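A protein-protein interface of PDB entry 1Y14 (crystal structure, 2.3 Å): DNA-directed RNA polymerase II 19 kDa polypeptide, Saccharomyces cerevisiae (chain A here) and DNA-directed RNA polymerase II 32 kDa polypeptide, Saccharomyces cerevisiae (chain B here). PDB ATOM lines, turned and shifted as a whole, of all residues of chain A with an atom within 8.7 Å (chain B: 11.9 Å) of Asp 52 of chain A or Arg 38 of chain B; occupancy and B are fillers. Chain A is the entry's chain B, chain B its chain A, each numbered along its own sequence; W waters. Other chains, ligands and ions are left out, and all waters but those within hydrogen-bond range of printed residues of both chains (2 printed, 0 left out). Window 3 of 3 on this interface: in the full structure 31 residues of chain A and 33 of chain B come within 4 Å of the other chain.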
ATOM      1  N   ARG A  21      21.266  24.216 -21.994  1.00  0.00           N
ATOM      2  CA  ARG A  21      20.411  23.346 -21.184  1.00  0.00           C
ATOM      3  C   ARG A  21      19.045  23.982 -20.912  1.00  0.00           C
ATOM      4  O   ARG A  21      18.187  23.374 -20.268  1.00  0.00           O
ATOM      5  CB  ARG A  21      21.094  23.035 -19.847  1.00  0.00           C
ATOM      6  CG  ARG A  21      22.150  21.945 -19.891  1.00  0.00           C
ATOM      7  CD  ARG A  21      21.519  20.559 -19.959  1.00  0.00           C
ATOM      8  NE  ARG A  21      22.523  19.501 -19.856  1.00  0.00           N
ATOM      9  CZ  ARG A  21      22.259  18.198 -19.935  1.00  0.00           C
ATOM     10  NH1 ARG A  21      21.013  17.775 -20.118  1.00  0.00           N
ATOM     11  NH2 ARG A  21      23.244  17.312 -19.833  1.00  0.00           N
ATOM     12  N   LYS A  23      16.525  24.217 -22.589  1.00  0.00           N
ATOM     13  CA  LYS A  23      15.385  23.471 -23.109  1.00  0.00           C
ATOM     14  C   LYS A  23      14.936  22.470 -22.055  1.00  0.00           C
ATOM     15  O   LYS A  23      13.750  22.391 -21.735  1.00  0.00           O
ATOM     16  CB  LYS A  23      15.745  22.747 -24.408  1.00  0.00           C
ATOM     17  CG  LYS A  23      15.803  23.675 -25.601  1.00  0.00           C
ATOM     18  CD  LYS A  23      16.077  22.927 -26.895  1.00  0.00           C
ATOM     19  CE  LYS A  23      16.130  23.892 -28.074  1.00  0.00           C
ATOM     20  NZ  LYS A  23      16.555  23.225 -29.330  1.00  0.00           N
ATOM     21  N   GLN A  24      15.883  21.711 -21.511  1.00  0.00           N
ATOM     22  CA  GLN A  24      15.554  20.739 -20.475  1.00  0.00           C
ATOM     23  C   GLN A  24      14.967  21.487 -19.281  1.00  0.00           C
ATOM     24  O   GLN A  24      14.147  20.947 -18.540  1.00  0.00           O
ATOM     25  CB  GLN A  24      16.801  19.969 -20.033  1.00  0.00           C
ATOM     26  CG  GLN A  24      16.569  19.033 -18.848  1.00  0.00           C
ATOM     27  CD  GLN A  24      17.835  18.305 -18.406  1.00  0.00           C
ATOM     28  OE1 GLN A  24      18.852  18.934 -18.102  1.00  0.00           O
ATOM     29  NE2 GLN A  24      17.773  16.976 -18.365  1.00  0.00           N
ATOM     30  N   LYS A  27      11.318  22.608 -19.963  1.00  0.00           N
ATOM     31  CA  LYS A  27      10.451  21.445 -19.829  1.00  0.00           C
ATOM     32  C   LYS A  27      10.166  21.165 -18.360  1.00  0.00           C
ATOM     33  O   LYS A  27       9.012  21.000 -17.965  1.00  0.00           O
ATOM     34  CB  LYS A  27      11.096  20.213 -20.467  1.00  0.00           C
ATOM     35  CG  LYS A  27      11.273  20.323 -21.975  1.00  0.00           C
ATOM     36  CD  LYS A  27      11.906  19.063 -22.555  1.00  0.00           C
ATOM     37  CE  LYS A  27      12.107  19.195 -24.053  1.00  0.00           C
ATOM     38  NZ  LYS A  27      12.810  18.016 -24.627  1.00  0.00           N
ATOM     39  N   VAL A  48       1.484  15.398 -19.236  1.00  0.00           N
ATOM     40  CA  VAL A  48       2.044  15.958 -20.460  1.00  0.00           C
ATOM     41  C   VAL A  48       2.629  14.772 -21.237  1.00  0.00           C
ATOM     42  O   VAL A  48       3.284  13.905 -20.670  1.00  0.00           O
ATOM     43  CB  VAL A  48       3.125  17.007 -20.132  1.00  0.00           C
ATOM     44  CG1 VAL A  48       3.800  17.505 -21.400  1.00  0.00           C
ATOM     45  CG2 VAL A  48       2.482  18.173 -19.406  1.00  0.00           C
ATOM     46  N   LEU A  49       2.361  14.732 -22.529  1.00  0.00           N
ATOM     47  CA  LEU A  49       2.807  13.626 -23.369  1.00  0.00           C
ATOM     48  C   LEU A  49       3.993  13.953 -24.251  1.00  0.00           C
ATOM     49  O   LEU A  49       4.377  15.115 -24.404  1.00  0.00           O
ATOM     50  CB  LEU A  49       1.669  13.192 -24.293  1.00  0.00           C
ATOM     51  CG  LEU A  49       0.288  12.999 -23.685  1.00  0.00           C
ATOM     52  CD1 LEU A  49      -0.688  12.712 -24.802  1.00  0.00           C
ATOM     53  CD2 LEU A  49       0.315  11.861 -22.669  1.00  0.00           C
ATOM     54  N   ASP A  50       4.566  12.905 -24.831  1.00  0.00           N
ATOM     55  CA  ASP A  50       5.657  13.065 -25.778  1.00  0.00           C
ATOM     56  C   ASP A  50       6.734  14.021 -25.285  1.00  0.00           C
ATOM     57  O   ASP A  50       7.028  15.034 -25.933  1.00  0.00           O
ATOM     58  CB  ASP A  50       5.054  13.564 -27.095  1.00  0.00           C
ATOM     59  CG  ASP A  50       6.034  13.527 -28.245  1.00  0.00           C
ATOM     60  OD1 ASP A  50       7.031  12.770 -28.161  1.00  0.00           O
ATOM     61  OD2 ASP A  50       5.789  14.247 -29.240  1.00  0.00           O
ATOM     62  N   TYR A  51       7.323  13.689 -24.138  1.00  0.00           N
ATOM     63  CA  TYR A  51       8.365  14.513 -23.528  1.00  0.00           C
ATOM     64  C   TYR A  51       9.472  14.961 -24.495  1.00  0.00           C
ATOM     65  O   TYR A  51       9.756  16.160 -24.628  1.00  0.00           O
ATOM     66  CB  TYR A  51       9.005  13.762 -22.357  1.00  0.00           C
ATOM     67  CG  TYR A  51       9.917  14.632 -21.511  1.00  0.00           C
ATOM     68  CD1 TYR A  51       9.405  15.400 -20.465  1.00  0.00           C
ATOM     69  CD2 TYR A  51      11.283  14.721 -21.785  1.00  0.00           C
ATOM     70  CE1 TYR A  51      10.232  16.236 -19.710  1.00  0.00           C
ATOM     71  CE2 TYR A  51      12.119  15.556 -21.037  1.00  0.00           C
ATOM     72  CZ  TYR A  51      11.587  16.310 -20.001  1.00  0.00           C
ATOM     73  OH  TYR A  51      12.405  17.136 -19.260  1.00  0.00           O
ATOM     74  N   ASP A  52      10.095  13.994 -25.168  1.00  0.00           N
ATOM     75  CA  ASP A  52      11.185  14.292 -26.093  1.00  0.00           C
ATOM     76  C   ASP A  52      10.831  15.224 -27.243  1.00  0.00           C
ATOM     77  O   ASP A  52      11.719  15.652 -27.970  1.00  0.00           O
ATOM     78  CB  ASP A  52      11.770  12.997 -26.675  1.00  0.00           C
ATOM     79  CG  ASP A  52      12.212  12.018 -25.603  1.00  0.00           C
ATOM     80  OD1 ASP A  52      12.759  12.472 -24.574  1.00  0.00           O
ATOM     81  OD2 ASP A  52      12.021  10.794 -25.791  1.00  0.00           O
ATOM     82  N   ASN A  53       9.554  15.559 -27.408  1.00  0.00           N
ATOM     83  CA  ASN A  53       9.162  16.427 -28.518  1.00  0.00           C
ATOM     84  C   ASN A  53       8.406  17.718 -28.183  1.00  0.00           C
ATOM     85  O   ASN A  53       7.831  18.358 -29.066  1.00  0.00           O
ATOM     86  CB  ASN A  53       8.371  15.610 -29.544  1.00  0.00           C
ATOM     87  CG  ASN A  53       9.234  14.572 -30.252  1.00  0.00           C
ATOM     88  OD1 ASN A  53      10.115  14.920 -31.041  1.00  0.00           O
ATOM     89  ND2 ASN A  53       8.993  13.295 -29.963  1.00  0.00           N
ATOM     90  N   ILE A  54       8.405  18.113 -26.918  1.00  0.00           N
ATOM     91  CA  ILE A  54       7.735  19.352 -26.540  1.00  0.00           C
ATOM     92  C   ILE A  54       8.315  20.500 -27.394  1.00  0.00           C
ATOM     93  O   ILE A  54       9.525  20.691 -27.437  1.00  0.00           O
ATOM     94  CB  ILE A  54       7.944  19.618 -25.032  1.00  0.00           C
ATOM     95  CG1 ILE A  54       7.287  18.487 -24.222  1.00  0.00           C
ATOM     96  CG2 ILE A  54       7.379  20.967 -24.661  1.00  0.00           C
ATOM     97  CD1 ILE A  54       7.518  18.540 -22.705  1.00  0.00           C
ATOM     98  N   ASP A  55       7.455  21.244 -28.086  1.00  0.00           N
ATOM     99  CA  ASP A  55       7.892  22.349 -28.954  1.00  0.00           C
ATOM    100  C   ASP A  55       8.143  23.684 -28.228  1.00  0.00           C
ATOM    101  O   ASP A  55       7.206  24.368 -27.814  1.00  0.00           O
ATOM    102  CB  ASP A  55       6.858  22.549 -30.067  1.00  0.00           C
ATOM    103  CG  ASP A  55       7.129  23.785 -30.902  1.00  0.00           C
ATOM    104  OD1 ASP A  55       8.256  23.922 -31.428  1.00  0.00           O
ATOM    105  OD2 ASP A  55       6.207  24.619 -31.039  1.00  0.00           O
ATOM    106  N   VAL B  24      -2.095   5.520 -23.263  1.00  0.00           N
ATOM    107  CA  VAL B  24      -1.436   6.776 -23.637  1.00  0.00           C
ATOM    108  C   VAL B  24      -0.589   7.343 -22.479  1.00  0.00           C
ATOM    109  O   VAL B  24       0.495   7.909 -22.691  1.00  0.00           O
ATOM    110  CB  VAL B  24      -2.477   7.829 -24.082  1.00  0.00           C
ATOM    111  CG1 VAL B  24      -1.827   9.200 -24.229  1.00  0.00           C
ATOM    112  CG2 VAL B  24      -3.101   7.398 -25.409  1.00  0.00           C
ATOM    113  N   LYS B  26       0.663   5.471 -19.722  1.00  0.00           N
ATOM    114  CA  LYS B  26       1.779   4.586 -19.398  1.00  0.00           C
ATOM    115  C   LYS B  26       2.925   4.794 -20.376  1.00  0.00           C
ATOM    116  O   LYS B  26       4.082   4.937 -19.981  1.00  0.00           O
ATOM    117  CB  LYS B  26       1.349   3.124 -19.428  1.00  0.00           C
ATOM    118  CG  LYS B  26       0.968   2.556 -18.076  1.00  0.00           C
ATOM    119  CD  LYS B  26       0.851   1.034 -18.148  1.00  0.00           C
ATOM    120  CE  LYS B  26       0.648   0.421 -16.770  1.00  0.00           C
ATOM    121  NZ  LYS B  26       0.542  -1.065 -16.832  1.00  0.00           N
ATOM    122  N   GLU B  27       2.589   4.826 -21.657  1.00  0.00           N
ATOM    123  CA  GLU B  27       3.583   5.023 -22.695  1.00  0.00           C
ATOM    124  C   GLU B  27       4.335   6.331 -22.469  1.00  0.00           C
ATOM    125  O   GLU B  27       5.560   6.371 -22.559  1.00  0.00           O
ATOM    126  CB  GLU B  27       2.906   5.045 -24.067  1.00  0.00           C
ATOM    127  CG  GLU B  27       3.846   5.341 -25.233  1.00  0.00           C
ATOM    128  CD  GLU B  27       3.105   5.774 -26.499  1.00  0.00           C
ATOM    129  OE1 GLU B  27       3.720   5.750 -27.588  1.00  0.00           O
ATOM    130  OE2 GLU B  27       1.915   6.149 -26.407  1.00  0.00           O
ATOM    131  N   ALA B  28       3.602   7.400 -22.169  1.00  0.00           N
ATOM    132  CA  ALA B  28       4.221   8.705 -21.955  1.00  0.00           C
ATOM    133  C   ALA B  28       5.175   8.666 -20.770  1.00  0.00           C
ATOM    134  O   ALA B  28       6.288   9.184 -20.854  1.00  0.00           O
ATOM    135  CB  ALA B  28       3.149   9.767 -21.725  1.00  0.00           C
ATOM    136  N   LEU B  29       4.745   8.047 -19.673  1.00  0.00           N
ATOM    137  CA  LEU B  29       5.590   7.969 -18.487  1.00  0.00           C
ATOM    138  C   LEU B  29       6.768   7.016 -18.677  1.00  0.00           C
ATOM    139  O   LEU B  29       7.845   7.251 -18.143  1.00  0.00           O
ATOM    140  CB  LEU B  29       4.768   7.558 -17.258  1.00  0.00           C
ATOM    141  CG  LEU B  29       3.669   8.555 -16.838  1.00  0.00           C
ATOM    142  CD1 LEU B  29       3.013   8.115 -15.543  1.00  0.00           C
ATOM    143  CD2 LEU B  29       4.266   9.940 -16.671  1.00  0.00           C
ATOM    144  N   VAL B  30       6.565   5.941 -19.433  1.00  0.00           N
ATOM    145  CA  VAL B  30       7.641   4.994 -19.680  1.00  0.00           C
ATOM    146  C   VAL B  30       8.752   5.698 -20.454  1.00  0.00           C
ATOM    147  O   VAL B  30       9.924   5.577 -20.120  1.00  0.00           O
ATOM    148  CB  VAL B  30       7.132   3.792 -20.480  1.00  0.00           C
ATOM    149  CG1 VAL B  30       8.299   3.035 -21.098  1.00  0.00           C
ATOM    150  CG2 VAL B  30       6.341   2.869 -19.554  1.00  0.00           C
ATOM    151  N   GLU B  31       8.359   6.446 -21.479  1.00  0.00           N
ATOM    152  CA  GLU B  31       9.276   7.203 -22.311  1.00  0.00           C
ATOM    153  C   GLU B  31       9.993   8.256 -21.473  1.00  0.00           C
ATOM    154  O   GLU B  31      11.168   8.537 -21.701  1.00  0.00           O
ATOM    155  CB  GLU B  31       8.503   7.893 -23.429  1.00  0.00           C
ATOM    156  CG  GLU B  31       9.347   8.702 -24.391  1.00  0.00           C
ATOM    157  CD  GLU B  31       8.498   9.554 -25.324  1.00  0.00           C
ATOM    158  OE1 GLU B  31       7.496   9.030 -25.864  1.00  0.00           O
ATOM    159  OE2 GLU B  31       8.836  10.746 -25.521  1.00  0.00           O
ATOM    160  N   ARG B  32       9.282   8.839 -20.510  1.00  0.00           N
ATOM    161  CA  ARG B  32       9.870   9.869 -19.659  1.00  0.00           C
ATOM    162  C   ARG B  32      10.895   9.246 -18.717  1.00  0.00           C
ATOM    163  O   ARG B  32      11.961   9.811 -18.481  1.00  0.00           O
ATOM    164  CB  ARG B  32       8.785  10.590 -18.853  1.00  0.00           C
ATOM    165  CG  ARG B  32       9.295  11.831 -18.132  1.00  0.00           C
ATOM    166  CD  ARG B  32       8.233  12.449 -17.232  1.00  0.00           C
ATOM    167  NE  ARG B  32       7.100  12.970 -17.992  1.00  0.00           N
ATOM    168  CZ  ARG B  32       6.035  13.551 -17.443  1.00  0.00           C
ATOM    169  NH1 ARG B  32       5.947  13.691 -16.122  1.00  0.00           N
ATOM    170  NH2 ARG B  32       5.055  13.989 -18.218  1.00  0.00           N
ATOM    171  N   ARG B  33      10.562   8.079 -18.182  1.00  0.00           N
ATOM    172  CA  ARG B  33      11.456   7.359 -17.289  1.00  0.00           C
ATOM    173  C   ARG B  33      12.782   7.126 -18.018  1.00  0.00           C
ATOM    174  O   ARG B  33      13.856   7.284 -17.439  1.00  0.00           O
ATOM    175  CB  ARG B  33      10.844   6.010 -16.897  1.00  0.00           C
ATOM    176  CG  ARG B  33      11.704   5.199 -15.941  1.00  0.00           C
ATOM    177  CD  ARG B  33      11.223   3.768 -15.867  1.00  0.00           C
ATOM    178  NE  ARG B  33      10.313   3.535 -14.750  1.00  0.00           N
ATOM    179  CZ  ARG B  33       9.507   2.480 -14.651  1.00  0.00           C
ATOM    180  NH1 ARG B  33       9.491   1.560 -15.609  1.00  0.00           N
ATOM    181  NH2 ARG B  33       8.728   2.334 -13.584  1.00  0.00           N
ATOM    182  N   ARG B  34      12.693   6.751 -19.293  1.00  0.00           N
ATOM    183  CA  ARG B  34      13.881   6.505 -20.102  1.00  0.00           C
ATOM    184  C   ARG B  34      14.631   7.803 -20.345  1.00  0.00           C
ATOM    185  O   ARG B  34      15.819   7.887 -20.070  1.00  0.00           O
ATOM    186  CB  ARG B  34      13.505   5.871 -21.447  1.00  0.00           C
ATOM    187  CG  ARG B  34      13.166   4.392 -21.356  1.00  0.00           C
ATOM    188  CD  ARG B  34      12.643   3.877 -22.687  1.00  0.00           C
ATOM    189  NE  ARG B  34      12.155   2.501 -22.597  1.00  0.00           N
ATOM    190  CZ  ARG B  34      11.229   1.989 -23.407  1.00  0.00           C
ATOM    191  NH1 ARG B  34      10.694   2.735 -24.366  1.00  0.00           N
ATOM    192  NH2 ARG B  34      10.821   0.739 -23.245  1.00  0.00           N
ATOM    193  N   ALA B  35      13.930   8.810 -20.864  1.00  0.00           N
ATOM    194  CA  ALA B  35      14.534  10.112 -21.133  1.00  0.00           C
ATOM    195  C   ALA B  35      15.265  10.601 -19.894  1.00  0.00           C
ATOM    196  O   ALA B  35      16.274  11.299 -19.992  1.00  0.00           O
ATOM    197  CB  ALA B  35      13.466  11.119 -21.535  1.00  0.00           C
ATOM    198  N   PHE B  36      14.754  10.234 -18.724  1.00  0.00           N
ATOM    199  CA  PHE B  36      15.389  10.630 -17.479  1.00  0.00           C
ATOM    200  C   PHE B  36      16.595   9.743 -17.183  1.00  0.00           C
ATOM    201  O   PHE B  36      17.669  10.251 -16.872  1.00  0.00           O
ATOM    202  CB  PHE B  36      14.388  10.586 -16.315  1.00  0.00           C
ATOM    203  CG  PHE B  36      13.412  11.745 -16.297  1.00  0.00           C
ATOM    204  CD1 PHE B  36      13.644  12.888 -17.060  1.00  0.00           C
ATOM    205  CD2 PHE B  36      12.276  11.702 -15.491  1.00  0.00           C
ATOM    206  CE1 PHE B  36      12.766  13.967 -17.021  1.00  0.00           C
ATOM    207  CE2 PHE B  36      11.389  12.779 -15.443  1.00  0.00           C
ATOM    208  CZ  PHE B  36      11.635  13.913 -16.210  1.00  0.00           C
ATOM    209  N   LYS B  37      16.423   8.424 -17.282  1.00  0.00           N
ATOM    210  CA  LYS B  37      17.521   7.485 -17.035  1.00  0.00           C
ATOM    211  C   LYS B  37      18.638   7.640 -18.065  1.00  0.00           C
ATOM    212  O   LYS B  37      19.772   7.226 -17.825  1.00  0.00           O
ATOM    213  CB  LYS B  37      17.027   6.037 -17.055  1.00  0.00           C
ATOM    214  CG  LYS B  37      16.317   5.605 -15.787  1.00  0.00           C
ATOM    215  CD  LYS B  37      15.865   4.153 -15.875  1.00  0.00           C
ATOM    216  CE  LYS B  37      15.078   3.734 -14.631  1.00  0.00           C
ATOM    217  NZ  LYS B  37      14.459   2.380 -14.763  1.00  0.00           N
ATOM    218  N   ARG B  38      18.310   8.224 -19.213  1.00  0.00           N
ATOM    219  CA  ARG B  38      19.294   8.450 -20.264  1.00  0.00           C
ATOM    220  C   ARG B  38      19.986   9.766 -19.957  1.00  0.00           C
ATOM    221  O   ARG B  38      20.649   9.913 -18.929  1.00  0.00           O
ATOM    222  CB  ARG B  38      18.636   8.590 -21.634  1.00  0.00           C
ATOM    223  CG  ARG B  38      17.859   7.412 -22.169  1.00  0.00           C
ATOM    224  CD  ARG B  38      16.879   7.970 -23.184  1.00  0.00           C
ATOM    225  NE  ARG B  38      17.508   9.053 -23.940  1.00  0.00           N
ATOM    226  CZ  ARG B  38      16.852  10.062 -24.504  1.00  0.00           C
ATOM    227  NH1 ARG B  38      15.532  10.143 -24.402  1.00  0.00           N
ATOM    228  NH2 ARG B  38      17.520  10.993 -25.175  1.00  0.00           N
ATOM    229  N   SER B  39      19.801  10.725 -20.864  1.00  0.00           N
ATOM    230  CA  SER B  39      20.389  12.054 -20.754  1.00  0.00           C
ATOM    231  C   SER B  39      20.362  12.585 -19.322  1.00  0.00           C
ATOM    232  O   SER B  39      19.344  13.098 -18.853  1.00  0.00           O
ATOM    233  CB  SER B  39      19.657  13.031 -21.682  1.00  0.00           C
ATOM    234  OG  SER B  39      20.242  14.323 -21.633  1.00  0.00           O
ATOM    235  N   GLN B  40      21.490  12.442 -18.632  1.00  0.00           N
ATOM    236  CA  GLN B  40      21.630  12.917 -17.263  1.00  0.00           C
ATOM    237  C   GLN B  40      22.866  13.803 -17.166  1.00  0.00           C
ATOM    238  O   GLN B  40      23.162  14.569 -18.087  1.00  0.00           O
ATOM    239  CB  GLN B  40      21.751  11.742 -16.284  1.00  0.00           C
ATOM    240  CG  GLN B  40      20.465  10.957 -16.108  1.00  0.00           C
ATOM    241  CD  GLN B  40      20.518   9.989 -14.941  1.00  0.00           C
ATOM    242  OE1 GLN B  40      21.340   9.075 -14.912  1.00  0.00           O
ATOM    243  NE2 GLN B  40      19.634  10.186 -13.968  1.00  0.00           N
ATOM    244  N   GLN B  98       9.284   7.801 -10.047  1.00  0.00           N
ATOM    245  CA  GLN B  98      10.407   8.076 -10.929  1.00  0.00           C
ATOM    246  C   GLN B  98      10.120   9.051 -12.056  1.00  0.00           C
ATOM    247  O   GLN B  98      11.040   9.498 -12.742  1.00  0.00           O
ATOM    248  CB  GLN B  98      10.902   6.764 -11.531  1.00  0.00           C
ATOM    249  CG  GLN B  98      11.043   5.635 -10.520  1.00  0.00           C
ATOM    250  CD  GLN B  98      11.383   4.307 -11.172  1.00  0.00           C
ATOM    251  OE1 GLN B  98      11.496   3.285 -10.500  1.00  0.00           O
ATOM    252  NE2 GLN B  98      11.550   4.319 -12.489  1.00  0.00           N
ATOM    253  N   THR B  99       8.857   9.397 -12.255  1.00  0.00           N
ATOM    254  CA  THR B  99       8.525  10.290 -13.355  1.00  0.00           C
ATOM    255  C   THR B  99       7.822  11.585 -12.998  1.00  0.00           C
ATOM    256  O   THR B  99       7.754  12.489 -13.828  1.00  0.00           O
ATOM    257  CB  THR B  99       7.659   9.557 -14.386  1.00  0.00           C
ATOM    258  OG1 THR B  99       6.464   9.097 -13.750  1.00  0.00           O
ATOM    259  CG2 THR B  99       8.416   8.345 -14.957  1.00  0.00           C
HETATM  260  O   HOH W   1       5.835  13.136 -20.961  1.00  0.00           O
HETATM  261  O   HOH W   2       6.919  10.899 -22.846  1.00  0.00           O
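O of Gln 40 of chain B lies within hydrogen-bond range of NH2 of Arg 21 of chain A.
The backbone carbonyl oxygen of Val 48 of chain A lies within hydrogen-bond range of the guanidinium group of Arg 32 of chain B, at 3.0 Å.
The guanidinium group of Arg 38 of chain B lies within salt-bridge range of the side-chain carboxylate of Asp 52 of chain A (3.6 Å).
The side-chain carboxylate of Asp 52 of chain A lies close to the side-chain carboxylate of Glu 31 of chain B.
NH1 of Arg 21 of chain A sits at hydrogen-bond distance from OE1 of Gln 24 of chain A, 3.2 Å away.
OD1 of Asp 50 of chain A lies within hydrogen-bond range of ND2 of Asn 53 of chain A, at 2.7 Å.
The guanidinium group (NH1) of Arg 32 of chain B sits at hydrogen-bond distance from the backbone carbonyl oxygen (O) of Thr 99 of chain B, at 3.2 Å.
Among the printed residues, merely in contact across the chains: Arg 21 of chain A with Ser 39 of chain B (3.8 Å), Leu 49 of chain A with Val 24 of chain B (3.7 Å), Leu 49 of chain A with Ala 28 of chain B (3.6 Å), Asp 50 of chain A with Glu 31 of chain B (3.8 Å), Tyr 51 of chain A with Glu 31 of chain B (3.6 Å), Tyr 51 of chain A with Phe 36 of chain B (3.9 Å) and Asp 52 of chain A with Ala 35 of chain B (3.4 Å).
Printed residues of chain B within 4 Å of Leu 49 of chain A: Val 24 (3.7 Å) and Ala 28 (3.6 Å).
Asp 50 of chain A touches just one residue of chain B: Glu 31 (3.8 Å).
Of the printed residues of chain B, Tyr 51 of chain A touches Glu 31 (3.6 Å) and Phe 36 (3.9 Å).
Asp 52 of chain A touches just these residues of chain B: Glu 31, Ala 35 and Arg 38.
Ile 54 of chain A touches none of the printed residues of chain B.
Of the printed residues of chain A, Ala 28 of chain B touches Leu 49 (3.6 Å).
Of the printed residues of chain A, Arg 32 of chain B touches Val 48 (3.0 Å).
Arg 34 of chain B touches none of the printed residues of chain A.
Ala 35 of chain B touches just one residue of chain A: Asp 52 (3.4 Å).
Arg 38 of chain B touches just one residue of chain A: Asp 52.
Printed residues of chain A within 4 Å of Ser 39 of chain B: Arg 21 (3.8 Å).
Printed residues of chain A within 4 Å of Gln 40 of chain B: Arg 21.
The nearest residue of chain B that does not touch Asp 52 of chain A is Arg 32 of chain B (6.3 Å).
Of the 18 printed residues of chain B, 9 touch a printed residue of chain A.
Printed residues of chain B that touch a printed residue of chain A: Val 24, Ala 28, Glu 31, Arg 32, Ala 35, Phe 36, Arg 38, Ser 39 and Gln 40.
Of the 12 printed residues of chain A, 6 touch a printed residue of chain B.
Among the printed residues, Asp or Glu carboxylates within 4 Å of a Lys or Arg side-chain nitrogen of the other chain: Asp 52 of chain A with Arg 38 of chain B.
Water W1 lies within hydrogen-bond range of O of Val 48 of chain A (2.7 Å) and NH2 of Arg 32 of chain B (3.0 Å).
Water W2 lies within hydrogen-bond range of O of Ala 28 of chain B, N of Tyr 51 of chain A and OE2 of Glu 31 of chain B.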
